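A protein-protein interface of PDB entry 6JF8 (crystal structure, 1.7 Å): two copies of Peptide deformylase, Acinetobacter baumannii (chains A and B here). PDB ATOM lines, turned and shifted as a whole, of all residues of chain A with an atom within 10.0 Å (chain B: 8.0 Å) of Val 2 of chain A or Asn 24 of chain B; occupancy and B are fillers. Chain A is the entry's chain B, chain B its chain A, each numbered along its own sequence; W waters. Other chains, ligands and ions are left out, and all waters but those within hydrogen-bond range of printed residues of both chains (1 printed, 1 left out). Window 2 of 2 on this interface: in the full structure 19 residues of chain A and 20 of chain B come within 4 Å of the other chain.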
ATOM      1  N   SER A   1      13.166  23.533  18.000  1.00  0.00           N
ATOM      2  CA  SER A   1      12.709  24.446  16.892  1.00  0.00           C
ATOM      3  C   SER A   1      11.599  23.833  16.020  1.00  0.00           C
ATOM      4  O   SER A   1      11.494  22.607  15.904  1.00  0.00           O
ATOM      5  CB  SER A   1      13.839  24.886  15.978  1.00  0.00           C
ATOM      6  OG  SER A   1      13.361  25.942  15.129  1.00  0.00           O
ATOM      7  N   VAL A   2      10.797  24.706  15.421  1.00  0.00           N
ATOM      8  CA  VAL A   2       9.583  24.301  14.667  1.00  0.00           C
ATOM      9  C   VAL A   2       9.485  25.162  13.453  1.00  0.00           C
ATOM     10  O   VAL A   2       9.948  26.301  13.505  1.00  0.00           O
ATOM     11  CB  VAL A   2       8.331  24.446  15.545  1.00  0.00           C
ATOM     12  CG1 VAL A   2       7.961  25.908  15.800  1.00  0.00           C
ATOM     13  CG2 VAL A   2       7.168  23.756  14.915  1.00  0.00           C
ATOM     14  N   VAL A   3       8.877  24.653  12.385  1.00  0.00           N
ATOM     15  CA  VAL A   3       8.498  25.388  11.188  1.00  0.00           C
ATOM     16  C   VAL A   3       6.988  25.199  11.109  1.00  0.00           C
ATOM     17  O   VAL A   3       6.505  24.107  11.052  1.00  0.00           O
ATOM     18  CB  VAL A   3       9.181  24.866   9.919  1.00  0.00           C
ATOM     19  CG1 VAL A   3       8.534  25.367   8.635  1.00  0.00           C
ATOM     20  CG2 VAL A   3      10.656  25.183   9.983  1.00  0.00           C
ATOM     21  N   LEU A   4       6.222  26.292  11.095  1.00  0.00           N
ATOM     22  CA  LEU A   4       4.777  26.232  11.140  1.00  0.00           C
ATOM     23  C   LEU A   4       4.148  26.199   9.753  1.00  0.00           C
ATOM     24  O   LEU A   4       4.690  26.838   8.871  1.00  0.00           O
ATOM     25  CB  LEU A   4       4.212  27.471  11.903  1.00  0.00           C
ATOM     26  CG  LEU A   4       4.611  27.534  13.353  1.00  0.00           C
ATOM     27  CD1 LEU A   4       4.216  28.911  13.909  1.00  0.00           C
ATOM     28  CD2 LEU A   4       3.986  26.351  14.121  1.00  0.00           C
ATOM     29  N   PRO A   5       3.024  25.492   9.562  1.00  0.00           N
ATOM     30  CA  PRO A   5       2.269  25.497   8.332  1.00  0.00           C
ATOM     31  C   PRO A   5       1.828  26.947   8.045  1.00  0.00           C
ATOM     32  O   PRO A   5       1.456  27.657   8.947  1.00  0.00           O
ATOM     33  CB  PRO A   5       1.046  24.645   8.597  1.00  0.00           C
ATOM     34  CG  PRO A   5       1.370  23.889   9.782  1.00  0.00           C
ATOM     35  CD  PRO A   5       2.475  24.507  10.514  1.00  0.00           C
ATOM     36  N   TYR A  32       7.533  34.748  23.381  1.00  0.00           N
ATOM     37  CA  TYR A  32       8.903  34.483  22.827  1.00  0.00           C
ATOM     38  C   TYR A  32       8.908  33.260  21.942  1.00  0.00           C
ATOM     39  O   TYR A  32       9.488  33.295  20.850  1.00  0.00           O
ATOM     40  CB  TYR A  32       9.988  34.320  23.921  1.00  0.00           C
ATOM     41  CG  TYR A  32      10.340  35.575  24.613  1.00  0.00           C
ATOM     42  CD1 TYR A  32      10.866  36.647  23.909  1.00  0.00           C
ATOM     43  CD2 TYR A  32      10.144  35.706  25.969  1.00  0.00           C
ATOM     44  CE1 TYR A  32      11.167  37.833  24.550  1.00  0.00           C
ATOM     45  CE2 TYR A  32      10.443  36.879  26.625  1.00  0.00           C
ATOM     46  CZ  TYR A  32      10.983  37.941  25.905  1.00  0.00           C
ATOM     47  OH  TYR A  32      11.285  39.136  26.524  1.00  0.00           O
ATOM     48  N   GLN A  33       8.231  32.162  22.335  1.00  0.00           N
ATOM     49  CA  GLN A  33       8.123  31.030  21.468  1.00  0.00           C
ATOM     50  C   GLN A  33       7.315  31.225  20.159  1.00  0.00           C
ATOM     51  O   GLN A  33       7.694  30.686  19.101  1.00  0.00           O
ATOM     52  CB  GLN A  33       7.512  29.820  22.256  1.00  0.00           C
ATOM     53  CG  GLN A  33       7.369  28.548  21.447  1.00  0.00           C
ATOM     54  CD  GLN A  33       8.701  27.992  20.930  1.00  0.00           C
ATOM     55  OE1 GLN A  33       9.566  27.651  21.743  1.00  0.00           O
ATOM     56  NE2 GLN A  33       8.881  27.931  19.573  1.00  0.00           N
ATOM     57  N   LEU A  34       6.167  31.898  20.231  1.00  0.00           N
ATOM     58  CA  LEU A  34       5.414  32.309  19.031  1.00  0.00           C
ATOM     59  C   LEU A  34       6.351  33.042  18.094  1.00  0.00           C
ATOM     60  O   LEU A  34       6.375  32.740  16.872  1.00  0.00           O
ATOM     61  CB  LEU A  34       4.131  33.165  19.339  1.00  0.00           C
ATOM     62  CG  LEU A  34       3.526  33.964  18.181  1.00  0.00           C
ATOM     63  CD1 LEU A  34       2.939  32.948  17.251  1.00  0.00           C
ATOM     64  CD2 LEU A  34       2.400  34.927  18.449  1.00  0.00           C
ATOM     65  N   ALA A  35       7.097  34.016  18.641  1.00  0.00           N
ATOM     66  CA  ALA A  35       7.909  34.895  17.782  1.00  0.00           C
ATOM     67  C   ALA A  35       9.060  34.059  17.170  1.00  0.00           C
ATOM     68  O   ALA A  35       9.338  34.127  15.965  1.00  0.00           O
ATOM     69  CB  ALA A  35       8.448  36.051  18.566  1.00  0.00           C
ATOM     70  N   ASP A  36       9.608  33.147  17.986  1.00  0.00           N
ATOM     71  CA  ASP A  36      10.629  32.247  17.465  1.00  0.00           C
ATOM     72  C   ASP A  36      10.148  31.295  16.380  1.00  0.00           C
ATOM     73  O   ASP A  36      10.861  31.032  15.434  1.00  0.00           O
ATOM     74  CB  ASP A  36      11.324  31.493  18.609  1.00  0.00           C
ATOM     75  CG  ASP A  36      12.482  30.648  18.125  1.00  0.00           C
ATOM     76  OD1 ASP A  36      13.466  31.214  17.597  1.00  0.00           O
ATOM     77  OD2 ASP A  36      12.373  29.404  18.229  1.00  0.00           O
ATOM     78  N   ALA A  37       8.980  30.715  16.546  1.00  0.00           N
ATOM     79  CA  ALA A  37       8.394  29.881  15.513  1.00  0.00           C
ATOM     80  C   ALA A  37       8.081  30.647  14.235  1.00  0.00           C
ATOM     81  O   ALA A  37       8.282  30.166  13.159  1.00  0.00           O
ATOM     82  CB  ALA A  37       7.131  29.228  16.033  1.00  0.00           C
ATOM     83  N   MET A  38       7.534  31.861  14.376  1.00  0.00           N
ATOM     84  CA  MET A  38       7.328  32.691  13.230  1.00  0.00           C
ATOM     85  C   MET A  38       8.658  32.958  12.470  1.00  0.00           C
ATOM     86  O   MET A  38       8.656  32.886  11.219  1.00  0.00           O
ATOM     87  CB  MET A  38       6.710  34.043  13.629  1.00  0.00           C
ATOM     88  CG  MET A  38       5.238  33.865  13.985  1.00  0.00           C
ATOM     89  SD  MET A  38       4.443  35.369  14.658  1.00  0.00           S
ATOM     90  CE  MET A  38       4.593  36.411  13.236  1.00  0.00           C
ATOM     91  N   HIS A  39       9.658  33.316  13.234  1.00  0.00           N
ATOM     92  CA  HIS A  39      10.981  33.697  12.687  1.00  0.00           C
ATOM     93  C   HIS A  39      11.576  32.512  11.916  1.00  0.00           C
ATOM     94  O   HIS A  39      11.957  32.628  10.762  1.00  0.00           O
ATOM     95  CB  HIS A  39      11.935  34.182  13.763  1.00  0.00           C
ATOM     96  CG  HIS A  39      13.190  34.796  13.209  1.00  0.00           C
ATOM     97  ND1 HIS A  39      13.383  36.150  13.087  1.00  0.00           N
ATOM     98  CD2 HIS A  39      14.320  34.225  12.745  1.00  0.00           C
ATOM     99  CE1 HIS A  39      14.577  36.391  12.577  1.00  0.00           C
ATOM    100  NE2 HIS A  39      15.167  35.242  12.364  1.00  0.00           N
ATOM    101  N   ALA A  40      11.535  31.348  12.550  1.00  0.00           N
ATOM    102  CA  ALA A  40      12.007  30.109  11.889  1.00  0.00           C
ATOM    103  C   ALA A  40      11.272  29.762  10.635  1.00  0.00           C
ATOM    104  O   ALA A  40      11.871  29.354   9.620  1.00  0.00           O
ATOM    105  CB  ALA A  40      11.932  28.926  12.882  1.00  0.00           C
ATOM    106  N   THR A  41       9.954  29.981  10.609  1.00  0.00           N
ATOM    107  CA  THR A  41       9.119  29.691   9.521  1.00  0.00           C
ATOM    108  C   THR A  41       9.405  30.644   8.340  1.00  0.00           C
ATOM    109  O   THR A  41       9.477  30.226   7.193  1.00  0.00           O
ATOM    110  CB  THR A  41       7.606  29.809   9.892  1.00  0.00           C
ATOM    111  OG1 THR A  41       7.298  28.875  10.941  1.00  0.00           O
ATOM    112  CG2 THR A  41       6.664  29.518   8.726  1.00  0.00           C
ATOM    113  N   MET A  42       9.510  31.926   8.663  1.00  0.00           N
ATOM    114  CA  MET A  42       9.914  32.934   7.679  1.00  0.00           C
ATOM    115  C   MET A  42      11.270  32.579   7.010  1.00  0.00           C
ATOM    116  O   MET A  42      11.336  32.563   5.796  1.00  0.00           O
ATOM    117  CB  MET A  42      10.050  34.272   8.383  1.00  0.00           C
ATOM    118  CG  MET A  42      10.365  35.420   7.418  1.00  0.00           C
ATOM    119  SD  MET A  42      10.731  36.918   8.428  1.00  0.00           S
ATOM    120  CE  MET A  42      12.308  36.474   9.144  1.00  0.00           C
ATOM    121  N   LEU A  43      12.241  32.224   7.838  1.00  0.00           N
ATOM    122  CA  LEU A  43      13.611  31.828   7.334  1.00  0.00           C
ATOM    123  C   LEU A  43      13.613  30.603   6.439  1.00  0.00           C
ATOM    124  O   LEU A  43      14.274  30.566   5.340  1.00  0.00           O
ATOM    125  CB  LEU A  43      14.577  31.636   8.486  1.00  0.00           C
ATOM    126  CG  LEU A  43      15.071  32.908   9.218  1.00  0.00           C
ATOM    127  CD1 LEU A  43      16.140  32.563  10.237  1.00  0.00           C
ATOM    128  CD2 LEU A  43      15.559  33.986   8.262  1.00  0.00           C
ATOM    129  N   GLU A  44      12.873  29.586   6.862  1.00  0.00           N
ATOM    130  CA  GLU A  44      12.777  28.370   6.088  1.00  0.00           C
ATOM    131  C   GLU A  44      12.092  28.598   4.762  1.00  0.00           C
ATOM    132  O   GLU A  44      12.459  27.964   3.772  1.00  0.00           O
ATOM    133  CB  GLU A  44      12.067  27.262   6.888  1.00  0.00           C
ATOM    134  CG  GLU A  44      11.897  25.907   6.164  1.00  0.00           C
ATOM    135  CD  GLU A  44      13.217  25.147   5.905  1.00  0.00           C
ATOM    136  OE1 GLU A  44      14.221  25.345   6.672  1.00  0.00           O
ATOM    137  OE2 GLU A  44      13.244  24.348   4.913  1.00  0.00           O
ATOM    138  N   ARG A  45      11.140  29.549   4.653  1.00  0.00           N
ATOM    139  CA  ARG A  45      10.472  29.778   3.388  1.00  0.00           C
ATOM    140  C   ARG A  45      11.063  30.963   2.595  1.00  0.00           C
ATOM    141  O   ARG A  45      10.426  31.359   1.609  1.00  0.00           O
ATOM    142  CB  ARG A  45       8.972  30.105   3.629  1.00  0.00           C
ATOM    143  CG  ARG A  45       8.131  29.171   4.512  1.00  0.00           C
ATOM    144  CD  ARG A  45       7.243  28.272   3.702  1.00  0.00           C
ATOM    145  NE  ARG A  45       8.085  27.236   3.132  1.00  0.00           N
ATOM    146  CZ  ARG A  45       8.453  26.088   3.738  1.00  0.00           C
ATOM    147  NH1 ARG A  45       8.064  25.771   4.967  1.00  0.00           N
ATOM    148  NH2 ARG A  45       9.239  25.231   3.089  1.00  0.00           N
ATOM    149  N   ILE A  50       6.825  38.267   8.005  1.00  0.00           N
ATOM    150  CA  ILE A  50       5.743  37.294   8.196  1.00  0.00           C
ATOM    151  C   ILE A  50       4.788  37.936   9.152  1.00  0.00           C
ATOM    152  O   ILE A  50       5.219  38.764   9.970  1.00  0.00           O
ATOM    153  CB  ILE A  50       6.279  35.948   8.740  1.00  0.00           C
ATOM    154  CG1 ILE A  50       5.215  34.841   8.555  1.00  0.00           C
ATOM    155  CG2 ILE A  50       6.925  36.126  10.094  1.00  0.00           C
ATOM    156  CD1 ILE A  50       5.834  33.429   8.792  1.00  0.00           C
ATOM    157  N   VAL A  55       0.358  32.046   9.911  1.00  0.00           N
ATOM    158  CA  VAL A  55       0.632  30.728  10.578  1.00  0.00           C
ATOM    159  C   VAL A  55      -0.544  30.269  11.504  1.00  0.00           C
ATOM    160  O   VAL A  55      -0.369  29.502  12.464  1.00  0.00           O
ATOM    161  CB  VAL A  55       1.990  30.637  11.199  1.00  0.00           C
ATOM    162  CG1 VAL A  55       3.113  30.703  10.184  1.00  0.00           C
ATOM    163  CG2 VAL A  55       2.163  31.670  12.309  1.00  0.00           C
ATOM    164  N   ILE A  57      -2.418  32.073  13.500  1.00  0.00           N
ATOM    165  CA  ILE A  57      -2.405  32.694  14.800  1.00  0.00           C
ATOM    166  C   ILE A  57      -3.018  34.085  14.575  1.00  0.00           C
ATOM    167  O   ILE A  57      -2.351  34.962  14.042  1.00  0.00           O
ATOM    168  CB  ILE A  57      -1.045  32.741  15.415  1.00  0.00           C
ATOM    169  CG1 ILE A  57      -0.506  31.299  15.575  1.00  0.00           C
ATOM    170  CG2 ILE A  57      -1.096  33.539  16.749  1.00  0.00           C
ATOM    171  CD1 ILE A  57       0.857  31.314  16.047  1.00  0.00           C
ATOM    172  N   VAL B  21      -2.950  20.252  13.506  1.00  0.00           N
ATOM    173  CA  VAL B  21      -1.556  20.435  13.936  1.00  0.00           C
ATOM    174  C   VAL B  21      -0.713  19.528  13.055  1.00  0.00           C
ATOM    175  O   VAL B  21      -1.062  18.370  12.818  1.00  0.00           O
ATOM    176  CB  VAL B  21      -1.427  20.041  15.447  1.00  0.00           C
ATOM    177  CG1 VAL B  21       0.038  20.080  15.923  1.00  0.00           C
ATOM    178  CG2 VAL B  21      -2.315  20.970  16.244  1.00  0.00           C
ATOM    179  N   SER B  22       0.419  20.038  12.604  1.00  0.00           N
ATOM    180  CA  SER B  22       1.246  19.386  11.635  1.00  0.00           C
ATOM    181  C   SER B  22       2.277  18.496  12.349  1.00  0.00           C
ATOM    182  O   SER B  22       2.517  18.615  13.535  1.00  0.00           O
ATOM    183  CB  SER B  22       1.991  20.375  10.796  1.00  0.00           C
ATOM    184  OG  SER B  22       2.974  21.114  11.504  1.00  0.00           O
ATOM    185  N   ALA B  23       2.805  17.608  11.588  1.00  0.00           N
ATOM    186  CA  ALA B  23       3.711  16.621  12.239  1.00  0.00           C
ATOM    187  C   ALA B  23       4.923  17.298  12.918  1.00  0.00           C
ATOM    188  O   ALA B  23       5.346  16.872  14.027  1.00  0.00           O
ATOM    189  CB  ALA B  23       4.216  15.671  11.136  1.00  0.00           C
ATOM    190  N   ASN B  24       5.488  18.331  12.280  1.00  0.00           N
ATOM    191  CA  ASN B  24       6.675  18.969  12.827  1.00  0.00           C
ATOM    192  C   ASN B  24       6.371  19.702  14.127  1.00  0.00           C
ATOM    193  O   ASN B  24       7.247  19.904  14.998  1.00  0.00           O
ATOM    194  CB  ASN B  24       7.395  19.914  11.844  1.00  0.00           C
ATOM    195  CG  ASN B  24       8.730  20.457  12.383  1.00  0.00           C
ATOM    196  OD1 ASN B  24       9.758  19.695  12.677  1.00  0.00           O
ATOM    197  ND2 ASN B  24       8.756  21.772  12.534  1.00  0.00           N
ATOM    198  N   GLU B  25       5.079  20.109  14.328  1.00  0.00           N
ATOM    199  CA  GLU B  25       4.665  20.672  15.597  1.00  0.00           C
ATOM    200  C   GLU B  25       4.568  19.696  16.763  1.00  0.00           C
ATOM    201  O   GLU B  25       4.568  20.133  17.851  1.00  0.00           O
ATOM    202  CB  GLU B  25       3.308  21.396  15.462  1.00  0.00           C
ATOM    203  CG  GLU B  25       3.377  22.578  14.529  1.00  0.00           C
ATOM    204  CD  GLU B  25       1.936  23.171  14.187  1.00  0.00           C
ATOM    205  OE1 GLU B  25       1.359  22.773  13.168  1.00  0.00           O
ATOM    206  OE2 GLU B  25       1.433  23.972  15.029  1.00  0.00           O
ATOM    207  N   LEU B  26       4.373  18.421  16.518  1.00  0.00           N
ATOM    208  CA  LEU B  26       4.214  17.456  17.544  1.00  0.00           C
ATOM    209  C   LEU B  26       5.532  17.385  18.335  1.00  0.00           C
ATOM    210  O   LEU B  26       6.620  17.532  17.745  1.00  0.00           O
ATOM    211  CB  LEU B  26       3.833  16.138  16.975  1.00  0.00           C
ATOM    212  CG  LEU B  26       2.598  15.963  16.161  1.00  0.00           C
ATOM    213  CD1 LEU B  26       2.495  14.563  15.631  1.00  0.00           C
ATOM    214  CD2 LEU B  26       1.441  16.377  17.060  1.00  0.00           C
ATOM    215  N   ASN B  27       5.395  17.313  19.654  1.00  0.00           N
ATOM    216  CA  ASN B  27       6.488  17.208  20.584  1.00  0.00           C
ATOM    217  C   ASN B  27       7.418  18.394  20.520  1.00  0.00           C
ATOM    218  O   ASN B  27       8.621  18.243  20.752  1.00  0.00           O
ATOM    219  CB  ASN B  27       7.255  15.906  20.310  1.00  0.00           C
ATOM    220  CG  ASN B  27       8.147  15.481  21.496  1.00  0.00           C
ATOM    221  OD1 ASN B  27       9.216  14.806  21.312  1.00  0.00           O
ATOM    222  ND2 ASN B  27       7.697  15.776  22.700  1.00  0.00           N
ATOM    223  N   SER B  28       6.903  19.567  20.155  1.00  0.00           N
ATOM    224  CA  SER B  28       7.615  20.847  20.071  1.00  0.00           C
ATOM    225  C   SER B  28       7.382  21.695  21.292  1.00  0.00           C
ATOM    226  O   SER B  28       6.316  21.682  21.964  1.00  0.00           O
ATOM    227  CB  SER B  28       7.250  21.597  18.775  1.00  0.00           C
ATOM    228  OG  SER B  28       5.918  22.184  18.871  1.00  0.00           O
ATOM    229  N   ASN B  29       8.379  22.524  21.623  1.00  0.00           N
ATOM    230  CA  ASN B  29       8.184  23.438  22.717  1.00  0.00           C
ATOM    231  C   ASN B  29       7.019  24.389  22.392  1.00  0.00           C
ATOM    232  O   ASN B  29       6.214  24.755  23.261  1.00  0.00           O
ATOM    233  CB  ASN B  29       9.465  24.265  22.925  1.00  0.00           C
ATOM    234  CG  ASN B  29       9.343  25.118  24.147  1.00  0.00           C
ATOM    235  OD1 ASN B  29       9.229  24.595  25.264  1.00  0.00           O
ATOM    236  ND2 ASN B  29       9.304  26.438  23.961  1.00  0.00           N
ATOM    237  N   TRP B  30       6.882  24.752  21.130  1.00  0.00           N
ATOM    238  CA  TRP B  30       5.749  25.542  20.657  1.00  0.00           C
ATOM    239  C   TRP B  30       4.414  24.938  21.113  1.00  0.00           C
ATOM    240  O   TRP B  30       3.585  25.607  21.743  1.00  0.00           O
ATOM    241  CB  TRP B  30       5.832  25.655  19.078  1.00  0.00           C
ATOM    242  CG  TRP B  30       4.517  25.821  18.384  1.00  0.00           C
ATOM    243  CD1 TRP B  30       3.925  24.909  17.597  1.00  0.00           C
ATOM    244  CD2 TRP B  30       3.647  26.933  18.440  1.00  0.00           C
ATOM    245  NE1 TRP B  30       2.687  25.338  17.178  1.00  0.00           N
ATOM    246  CE2 TRP B  30       2.496  26.594  17.675  1.00  0.00           C
ATOM    247  CE3 TRP B  30       3.698  28.167  19.100  1.00  0.00           C
ATOM    248  CZ2 TRP B  30       1.420  27.449  17.511  1.00  0.00           C
ATOM    249  CZ3 TRP B  30       2.606  29.025  18.989  1.00  0.00           C
ATOM    250  CH2 TRP B  30       1.460  28.652  18.201  1.00  0.00           C
ATOM    251  N   LEU B  31       4.221  23.666  20.832  1.00  0.00           N
ATOM    252  CA  LEU B  31       2.932  23.042  21.148  1.00  0.00           C
ATOM    253  C   LEU B  31       2.733  22.898  22.668  1.00  0.00           C
ATOM    254  O   LEU B  31       1.646  23.080  23.193  1.00  0.00           O
ATOM    255  CB  LEU B  31       2.877  21.709  20.456  1.00  0.00           C
ATOM    256  CG  LEU B  31       1.554  20.947  20.521  1.00  0.00           C
ATOM    257  CD1 LEU B  31       0.511  21.859  19.930  1.00  0.00           C
ATOM    258  CD2 LEU B  31       1.602  19.584  19.780  1.00  0.00           C
HETATM  259  O   HOH W   1       5.018  22.053  10.087  1.00  0.00           O
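Water W1 bridges the side-chain hydroxyl of Ser 22 of chain B and the backbone carbonyl oxygen of Val 3 of chain A.
Among the printed residues, pairs that only touch across the chains: Pro 5 of chain A with Glu 25 of chain B, Val 2 of chain A with Asn 24 of chain B, Leu 4 of chain A with Trp 30 of chain B, Ile 57 of chain A with Trp 30 of chain B, Gln 33 of chain A with Trp 30 of chain B, Pro 5 of chain A with Ser 22 of chain B, Leu 4 of chain A with Glu 25 of chain B, Val 2 of chain A with Trp 30 of chain B and Val 2 of chain A with Glu 25 of chain B.
The backbone NH (N) of Val 3 of chain A sits close to the side-chain amide nitrogen (ND2) of Asn 24 of chain B (2.9 Å).
The side-chain amide nitrogen of Asn 29 of chain B lies within hydrogen-bond range of the side-chain amide oxygen of Gln 33 of chain A (2.5 Å).
Of the 11 printed residues of chain B, 5 touch a printed residue of chain A.
Hydrophobic or aromatic side chains of chain B within 4 Å of the printed part of chain A: Trp 30.
Of the 22 printed residues of chain A, 6 touch a printed residue of chain B.
Hydrophobic or aromatic side chains of chain A within 4 Å of the printed part of chain B: Val 2, Leu 4, Pro 5 and Ile 57.
Printed residues of chain B within 4 Å of Val 2 of chain A: Asn 24 (3.4 Å), Glu 25 (3.99 Å) and Trp 30 (3.9 Å).
Of the printed residues of chain B, Val 3 of chain A touches Asn 24 (2.9 Å).
Printed residues of chain B within 4 Å of Leu 4 of chain A: Glu 25 (3.6 Å) and Trp 30 (3.5 Å).
Of the printed residues of chain B, Gln 33 of chain A touches Asn 29 (2.5 Å) and Trp 30 (3.5 Å).
Printed residues of chain A within 4 Å of Ser 22 of chain B: Pro 5.
No residue of chain A comes within 4 Å of Ala 23 of chain B.
Printed residues of chain A within 4 Å of Asn 24 of chain B: Val 2 (3.4 Å) and Val 3 (2.9 Å).
Leu 26 of chain B touches none of the printed residues of chain A.
Of the printed residues of chain A, Trp 30 of chain B touches Val 2, Leu 4, Gln 33 and Ile 57.
The nearest residue of chain A that does not touch Asn 24 of chain B is Ser 1 of chain A (4.4 Å).
The nearest printed residue of chain B that does not touch Leu 4 of chain A is Asn 24 of chain B (5.4 Å).
OG of Ser 22 of chain B is in hydrogen-bond range of OE1 of Glu 25 of chain B (2.9 Å).
The backbone carbonyl oxygen (O) of Glu 25 of chain B sits at hydrogen-bond distance from the side-chain hydroxyl (OG) of Ser 28 of chain B (2.7 Å).
The indole nitrogen of Trp 30 of chain B lies within hydrogen-bond range of the side-chain carboxylate of Glu 25 of chain B (2.8 Å).
The backbone NH of Leu 4 of chain A sits at hydrogen-bond distance from the side-chain hydroxyl of Thr 41 of chain A (2.8 Å).
No position is printed for both chains.
Of the 11 pairs that touch across the chains among the printed residues, none has its exchanged pair printed and touching as well.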
